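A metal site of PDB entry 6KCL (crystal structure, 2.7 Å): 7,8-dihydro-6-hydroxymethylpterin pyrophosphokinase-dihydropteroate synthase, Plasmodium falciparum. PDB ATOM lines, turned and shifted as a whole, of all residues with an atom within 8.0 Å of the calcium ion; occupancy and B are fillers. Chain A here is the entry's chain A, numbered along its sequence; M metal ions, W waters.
The calcium ion is bound by water W2 (2.2 Å), O of Glu 42 (2.3 Å), OE1 of Glu 99 (2.4 Å), water W1 (2.5 Å), O of Gly 46 (2.5 Å), OE2 of Glu 99 (2.6 Å) and OE1 of Glu 42 (2.6 Å).
The side-chain carboxylate (OE2) of Glu 42 is in hydrogen-bond range of the backbone NH (N) of Ile 48 (2.9 Å).
Three residues have an atom within 4 Å of the calcium ion: Glu 42, Gly 46 and Glu 99.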
ATOM      1  N   LEU A  38      -7.430  19.972   9.904  1.00  0.00           N
ATOM      2  CA  LEU A  38      -6.735  21.049  10.635  1.00  0.00           C
ATOM      3  C   LEU A  38      -7.699  22.104  11.174  1.00  0.00           C
ATOM      4  O   LEU A  38      -7.485  22.608  12.271  1.00  0.00           O
ATOM      5  CB  LEU A  38      -5.606  21.702   9.789  1.00  0.00           C
ATOM      6  CG  LEU A  38      -4.341  20.884   9.452  1.00  0.00           C
ATOM      7  CD1 LEU A  38      -3.460  21.645   8.487  1.00  0.00           C
ATOM      8  CD2 LEU A  38      -3.515  20.488  10.663  1.00  0.00           C
ATOM      9  N   HIS A  39      -8.772  22.424  10.430  1.00  0.00           N
ATOM     10  CA  HIS A  39      -9.732  23.442  10.873  1.00  0.00           C
ATOM     11  C   HIS A  39     -10.440  22.947  12.079  1.00  0.00           C
ATOM     12  O   HIS A  39     -10.668  23.701  13.039  1.00  0.00           O
ATOM     13  CB  HIS A  39     -10.755  23.802   9.802  1.00  0.00           C
ATOM     14  CG  HIS A  39     -10.182  24.548   8.609  1.00  0.00           C
ATOM     15  ND1 HIS A  39      -9.377  25.634   8.739  1.00  0.00           N
ATOM     16  CD2 HIS A  39     -10.371  24.357   7.234  1.00  0.00           C
ATOM     17  CE1 HIS A  39      -9.048  26.102   7.500  1.00  0.00           C
ATOM     18  NE2 HIS A  39      -9.660  25.311   6.588  1.00  0.00           N
ATOM     19  N   LEU A  40     -10.802  21.655  12.036  1.00  0.00           N
ATOM     20  CA  LEU A  40     -11.576  21.040  13.113  1.00  0.00           C
ATOM     21  C   LEU A  40     -10.719  20.833  14.347  1.00  0.00           C
ATOM     22  O   LEU A  40     -11.200  21.021  15.467  1.00  0.00           O
ATOM     23  CB  LEU A  40     -12.268  19.771  12.636  1.00  0.00           C
ATOM     24  CG  LEU A  40     -13.312  20.086  11.533  1.00  0.00           C
ATOM     25  CD1 LEU A  40     -13.943  18.851  10.910  1.00  0.00           C
ATOM     26  CD2 LEU A  40     -14.395  21.020  12.053  1.00  0.00           C
ATOM     27  N   VAL A  41      -9.441  20.532  14.117  1.00  0.00           N
ATOM     28  CA  VAL A  41      -8.466  20.528  15.199  1.00  0.00           C
ATOM     29  C   VAL A  41      -8.422  21.900  15.850  1.00  0.00           C
ATOM     30  O   VAL A  41      -8.527  21.962  17.070  1.00  0.00           O
ATOM     31  CB  VAL A  41      -7.055  20.085  14.735  1.00  0.00           C
ATOM     32  CG1 VAL A  41      -6.006  20.383  15.816  1.00  0.00           C
ATOM     33  CG2 VAL A  41      -7.041  18.611  14.358  1.00  0.00           C
ATOM     34  N   GLU A  42      -8.273  22.976  15.071  1.00  0.00           N
ATOM     35  CA  GLU A  42      -8.223  24.360  15.632  1.00  0.00           C
ATOM     36  C   GLU A  42      -9.486  24.729  16.379  1.00  0.00           C
ATOM     37  O   GLU A  42      -9.445  25.471  17.353  1.00  0.00           O
ATOM     38  CB  GLU A  42      -8.014  25.452  14.571  1.00  0.00           C
ATOM     39  CG  GLU A  42      -6.577  25.870  14.318  1.00  0.00           C
ATOM     40  CD  GLU A  42      -5.970  26.780  15.388  1.00  0.00           C
ATOM     41  OE1 GLU A  42      -6.696  27.307  16.280  1.00  0.00           O
ATOM     42  OE2 GLU A  42      -4.727  27.001  15.307  1.00  0.00           O
ATOM     43  N   LYS A  43     -10.611  24.217  15.882  1.00  0.00           N
ATOM     44  CA  LYS A  43     -11.902  24.580  16.410  1.00  0.00           C
ATOM     45  C   LYS A  43     -12.237  23.778  17.643  1.00  0.00           C
ATOM     46  O   LYS A  43     -12.751  24.339  18.588  1.00  0.00           O
ATOM     47  CB  LYS A  43     -12.971  24.383  15.346  1.00  0.00           C
ATOM     48  CG  LYS A  43     -14.384  24.726  15.753  1.00  0.00           C
ATOM     49  CD  LYS A  43     -15.314  24.308  14.612  1.00  0.00           C
ATOM     50  CE  LYS A  43     -16.776  24.708  14.830  1.00  0.00           C
ATOM     51  NZ  LYS A  43     -16.995  26.166  14.606  1.00  0.00           N
ATOM     52  N   TYR A  44     -11.959  22.480  17.622  1.00  0.00           N
ATOM     53  CA  TYR A  44     -12.444  21.593  18.676  1.00  0.00           C
ATOM     54  C   TYR A  44     -11.411  21.215  19.755  1.00  0.00           C
ATOM     55  O   TYR A  44     -11.794  20.845  20.865  1.00  0.00           O
ATOM     56  CB  TYR A  44     -13.110  20.337  18.099  1.00  0.00           C
ATOM     57  CG  TYR A  44     -14.431  20.604  17.392  1.00  0.00           C
ATOM     58  CD1 TYR A  44     -15.369  21.483  17.939  1.00  0.00           C
ATOM     59  CD2 TYR A  44     -14.737  19.977  16.191  1.00  0.00           C
ATOM     60  CE1 TYR A  44     -16.560  21.745  17.290  1.00  0.00           C
ATOM     61  CE2 TYR A  44     -15.936  20.228  15.538  1.00  0.00           C
ATOM     62  CZ  TYR A  44     -16.839  21.108  16.093  1.00  0.00           C
ATOM     63  OH  TYR A  44     -18.050  21.370  15.455  1.00  0.00           O
ATOM     64  N   LEU A  45     -10.125  21.321  19.446  1.00  0.00           N
ATOM     65  CA  LEU A  45      -9.110  20.764  20.338  1.00  0.00           C
ATOM     66  C   LEU A  45      -8.223  21.773  21.031  1.00  0.00           C
ATOM     67  O   LEU A  45      -7.745  21.509  22.130  1.00  0.00           O
ATOM     68  CB  LEU A  45      -8.234  19.739  19.584  1.00  0.00           C
ATOM     69  CG  LEU A  45      -8.983  18.516  19.052  1.00  0.00           C
ATOM     70  CD1 LEU A  45      -8.080  17.631  18.207  1.00  0.00           C
ATOM     71  CD2 LEU A  45      -9.577  17.751  20.216  1.00  0.00           C
ATOM     72  N   GLY A  46      -7.999  22.912  20.404  1.00  0.00           N
ATOM     73  CA  GLY A  46      -7.070  23.913  20.931  1.00  0.00           C
ATOM     74  C   GLY A  46      -6.421  24.742  19.836  1.00  0.00           C
ATOM     75  O   GLY A  46      -7.076  25.126  18.844  1.00  0.00           O
ATOM     76  N   LYS A  47      -5.126  25.005  20.002  1.00  0.00           N
ATOM     77  CA  LYS A  47      -4.391  25.873  19.103  1.00  0.00           C
ATOM     78  C   LYS A  47      -3.314  25.073  18.396  1.00  0.00           C
ATOM     79  O   LYS A  47      -2.533  24.377  19.038  1.00  0.00           O
ATOM     80  CB  LYS A  47      -3.763  27.039  19.868  1.00  0.00           C
ATOM     81  CG  LYS A  47      -3.071  28.042  18.956  1.00  0.00           C
ATOM     82  CD  LYS A  47      -2.617  29.280  19.695  1.00  0.00           C
ATOM     83  CE  LYS A  47      -1.844  30.237  18.798  1.00  0.00           C
ATOM     84  NZ  LYS A  47      -2.693  30.713  17.644  1.00  0.00           N
ATOM     85  N   ILE A  48      -3.276  25.176  17.075  1.00  0.00           N
ATOM     86  CA  ILE A  48      -2.181  24.576  16.312  1.00  0.00           C
ATOM     87  C   ILE A  48      -0.949  25.466  16.436  1.00  0.00           C
ATOM     88  O   ILE A  48      -1.007  26.640  16.105  1.00  0.00           O
ATOM     89  CB  ILE A  48      -2.573  24.361  14.845  1.00  0.00           C
ATOM     90  CG1 ILE A  48      -3.722  23.342  14.772  1.00  0.00           C
ATOM     91  CG2 ILE A  48      -1.360  23.954  14.004  1.00  0.00           C
ATOM     92  CD1 ILE A  48      -4.359  23.221  13.404  1.00  0.00           C
ATOM     93  N   SER A  95     -17.819  25.053  19.324  1.00  0.00           N
ATOM     94  CA  SER A  95     -17.023  24.604  20.447  1.00  0.00           C
ATOM     95  C   SER A  95     -17.472  25.403  21.649  1.00  0.00           C
ATOM     96  O   SER A  95     -18.084  26.450  21.490  1.00  0.00           O
ATOM     97  CB  SER A  95     -15.523  24.841  20.204  1.00  0.00           C
ATOM     98  OG  SER A  95     -14.783  24.757  21.419  1.00  0.00           O
ATOM     99  N   TYR A  97     -15.144  26.259  23.716  1.00  0.00           N
ATOM    100  CA  TYR A  97     -13.908  26.945  24.029  1.00  0.00           C
ATOM    101  C   TYR A  97     -13.611  28.043  23.018  1.00  0.00           C
ATOM    102  O   TYR A  97     -13.876  27.892  21.824  1.00  0.00           O
ATOM    103  CB  TYR A  97     -12.741  25.972  24.154  1.00  0.00           C
ATOM    104  CG  TYR A  97     -12.796  25.175  25.433  1.00  0.00           C
ATOM    105  CD1 TYR A  97     -13.751  24.156  25.601  1.00  0.00           C
ATOM    106  CD2 TYR A  97     -11.903  25.436  26.495  1.00  0.00           C
ATOM    107  CE1 TYR A  97     -13.817  23.423  26.771  1.00  0.00           C
ATOM    108  CE2 TYR A  97     -11.978  24.699  27.667  1.00  0.00           C
ATOM    109  CZ  TYR A  97     -12.935  23.707  27.788  1.00  0.00           C
ATOM    110  OH  TYR A  97     -13.017  22.949  28.935  1.00  0.00           O
ATOM    111  N   GLU A  98     -13.061  29.130  23.539  1.00  0.00           N
ATOM    112  CA  GLU A  98     -12.738  30.338  22.797  1.00  0.00           C
ATOM    113  C   GLU A  98     -11.771  30.091  21.668  1.00  0.00           C
ATOM    114  O   GLU A  98     -10.760  29.386  21.843  1.00  0.00           O
ATOM    115  CB  GLU A  98     -12.032  31.310  23.745  1.00  0.00           C
ATOM    116  CG  GLU A  98     -12.949  32.173  24.581  1.00  0.00           C
ATOM    117  CD  GLU A  98     -12.163  33.051  25.538  1.00  0.00           C
ATOM    118  OE1 GLU A  98     -10.921  32.866  25.614  1.00  0.00           O
ATOM    119  OE2 GLU A  98     -12.813  33.903  26.199  1.00  0.00           O
ATOM    120  N   GLU A  99     -12.034  30.690  20.510  1.00  0.00           N
ATOM    121  CA  GLU A  99     -10.977  30.899  19.549  1.00  0.00           C
ATOM    122  C   GLU A  99     -10.260  32.238  19.844  1.00  0.00           C
ATOM    123  O   GLU A  99     -10.890  33.222  20.235  1.00  0.00           O
ATOM    124  CB  GLU A  99     -11.545  30.879  18.147  1.00  0.00           C
ATOM    125  CG  GLU A  99     -10.483  30.752  17.078  1.00  0.00           C
ATOM    126  CD  GLU A  99      -9.638  29.504  17.257  1.00  0.00           C
ATOM    127  OE1 GLU A  99      -8.579  29.597  17.939  1.00  0.00           O
ATOM    128  OE2 GLU A  99     -10.058  28.433  16.740  1.00  0.00           O
ATOM    129  N   ASN A 100      -8.939  32.254  19.695  1.00  0.00           N
ATOM    130  CA  ASN A 100      -8.168  33.485  19.866  1.00  0.00           C
ATOM    131  C   ASN A 100      -7.147  33.566  18.793  1.00  0.00           C
ATOM    132  O   ASN A 100      -6.234  32.744  18.764  1.00  0.00           O
ATOM    133  CB  ASN A 100      -7.480  33.550  21.204  1.00  0.00           C
ATOM    134  CG  ASN A 100      -8.457  33.637  22.359  1.00  0.00           C
ATOM    135  OD1 ASN A 100      -9.518  34.268  22.255  1.00  0.00           O
ATOM    136  ND2 ASN A 100      -8.119  33.000  23.474  1.00  0.00           N
ATOM    137  N   LYS A 101      -7.271  34.543  17.909  1.00  0.00           N
ATOM    138  CA  LYS A 101      -6.349  34.653  16.805  1.00  0.00           C
ATOM    139  C   LYS A 101      -5.156  35.552  17.108  1.00  0.00           C
ATOM    140  O   LYS A 101      -4.253  35.635  16.294  1.00  0.00           O
ATOM    141  CB  LYS A 101      -7.088  35.061  15.512  1.00  0.00           C
ATOM    142  CG  LYS A 101      -8.054  33.975  15.039  1.00  0.00           C
ATOM    143  CD  LYS A 101      -9.082  34.447  14.025  1.00  0.00           C
ATOM    144  CE  LYS A 101      -8.723  34.020  12.600  1.00  0.00           C
ATOM    145  NZ  LYS A 101      -7.628  34.786  11.924  1.00  0.00           N
ATOM    146  N   VAL A 170      -0.587  20.507  19.005  1.00  0.00           N
ATOM    147  CA  VAL A 170      -1.758  21.222  19.487  1.00  0.00           C
ATOM    148  C   VAL A 170      -1.582  21.586  20.953  1.00  0.00           C
ATOM    149  O   VAL A 170      -1.303  20.725  21.764  1.00  0.00           O
ATOM    150  CB  VAL A 170      -3.059  20.424  19.347  1.00  0.00           C
ATOM    151  CG1 VAL A 170      -4.241  21.339  19.517  1.00  0.00           C
ATOM    152  CG2 VAL A 170      -3.151  19.786  17.988  1.00  0.00           C
ATOM    153  N   LYS A 171      -1.727  22.865  21.252  1.00  0.00           N
ATOM    154  CA  LYS A 171      -1.830  23.316  22.615  1.00  0.00           C
ATOM    155  C   LYS A 171      -3.295  23.131  22.917  1.00  0.00           C
ATOM    156  O   LYS A 171      -4.149  23.846  22.386  1.00  0.00           O
ATOM    157  CB  LYS A 171      -1.418  24.773  22.668  1.00  0.00           C
ATOM    158  CG  LYS A 171      -1.478  25.439  24.012  1.00  0.00           C
ATOM    159  CD  LYS A 171      -1.132  26.907  23.770  1.00  0.00           C
ATOM    160  CE  LYS A 171      -0.449  27.564  24.952  1.00  0.00           C
ATOM    161  NZ  LYS A 171       0.366  28.702  24.433  1.00  0.00           N
ATOM    162  N   PHE A 173      -6.854  22.262  25.235  1.00  0.00           N
ATOM    163  CA  PHE A 173      -7.602  22.481  26.476  1.00  0.00           C
ATOM    164  C   PHE A 173      -8.303  21.194  26.904  1.00  0.00           C
ATOM    165  O   PHE A 173      -8.899  21.143  27.972  1.00  0.00           O
ATOM    166  CB  PHE A 173      -8.639  23.596  26.271  1.00  0.00           C
ATOM    167  CG  PHE A 173      -9.390  23.511  24.968  1.00  0.00           C
ATOM    168  CD1 PHE A 173     -10.275  22.441  24.720  1.00  0.00           C
ATOM    169  CD2 PHE A 173      -9.222  24.487  23.984  1.00  0.00           C
ATOM    170  CE1 PHE A 173     -10.958  22.357  23.514  1.00  0.00           C
ATOM    171  CE2 PHE A 173      -9.895  24.407  22.776  1.00  0.00           C
ATOM    172  CZ  PHE A 173     -10.767  23.335  22.532  1.00  0.00           C
HETATM  173 CA    CA M   1      -8.375  27.224  18.314  1.00  0.00          CA
HETATM  174  O   HOH W   1     -10.161  27.494  19.972  1.00  0.00           O
HETATM  175  O   HOH W   2      -7.193  27.909  20.074  1.00  0.00           O
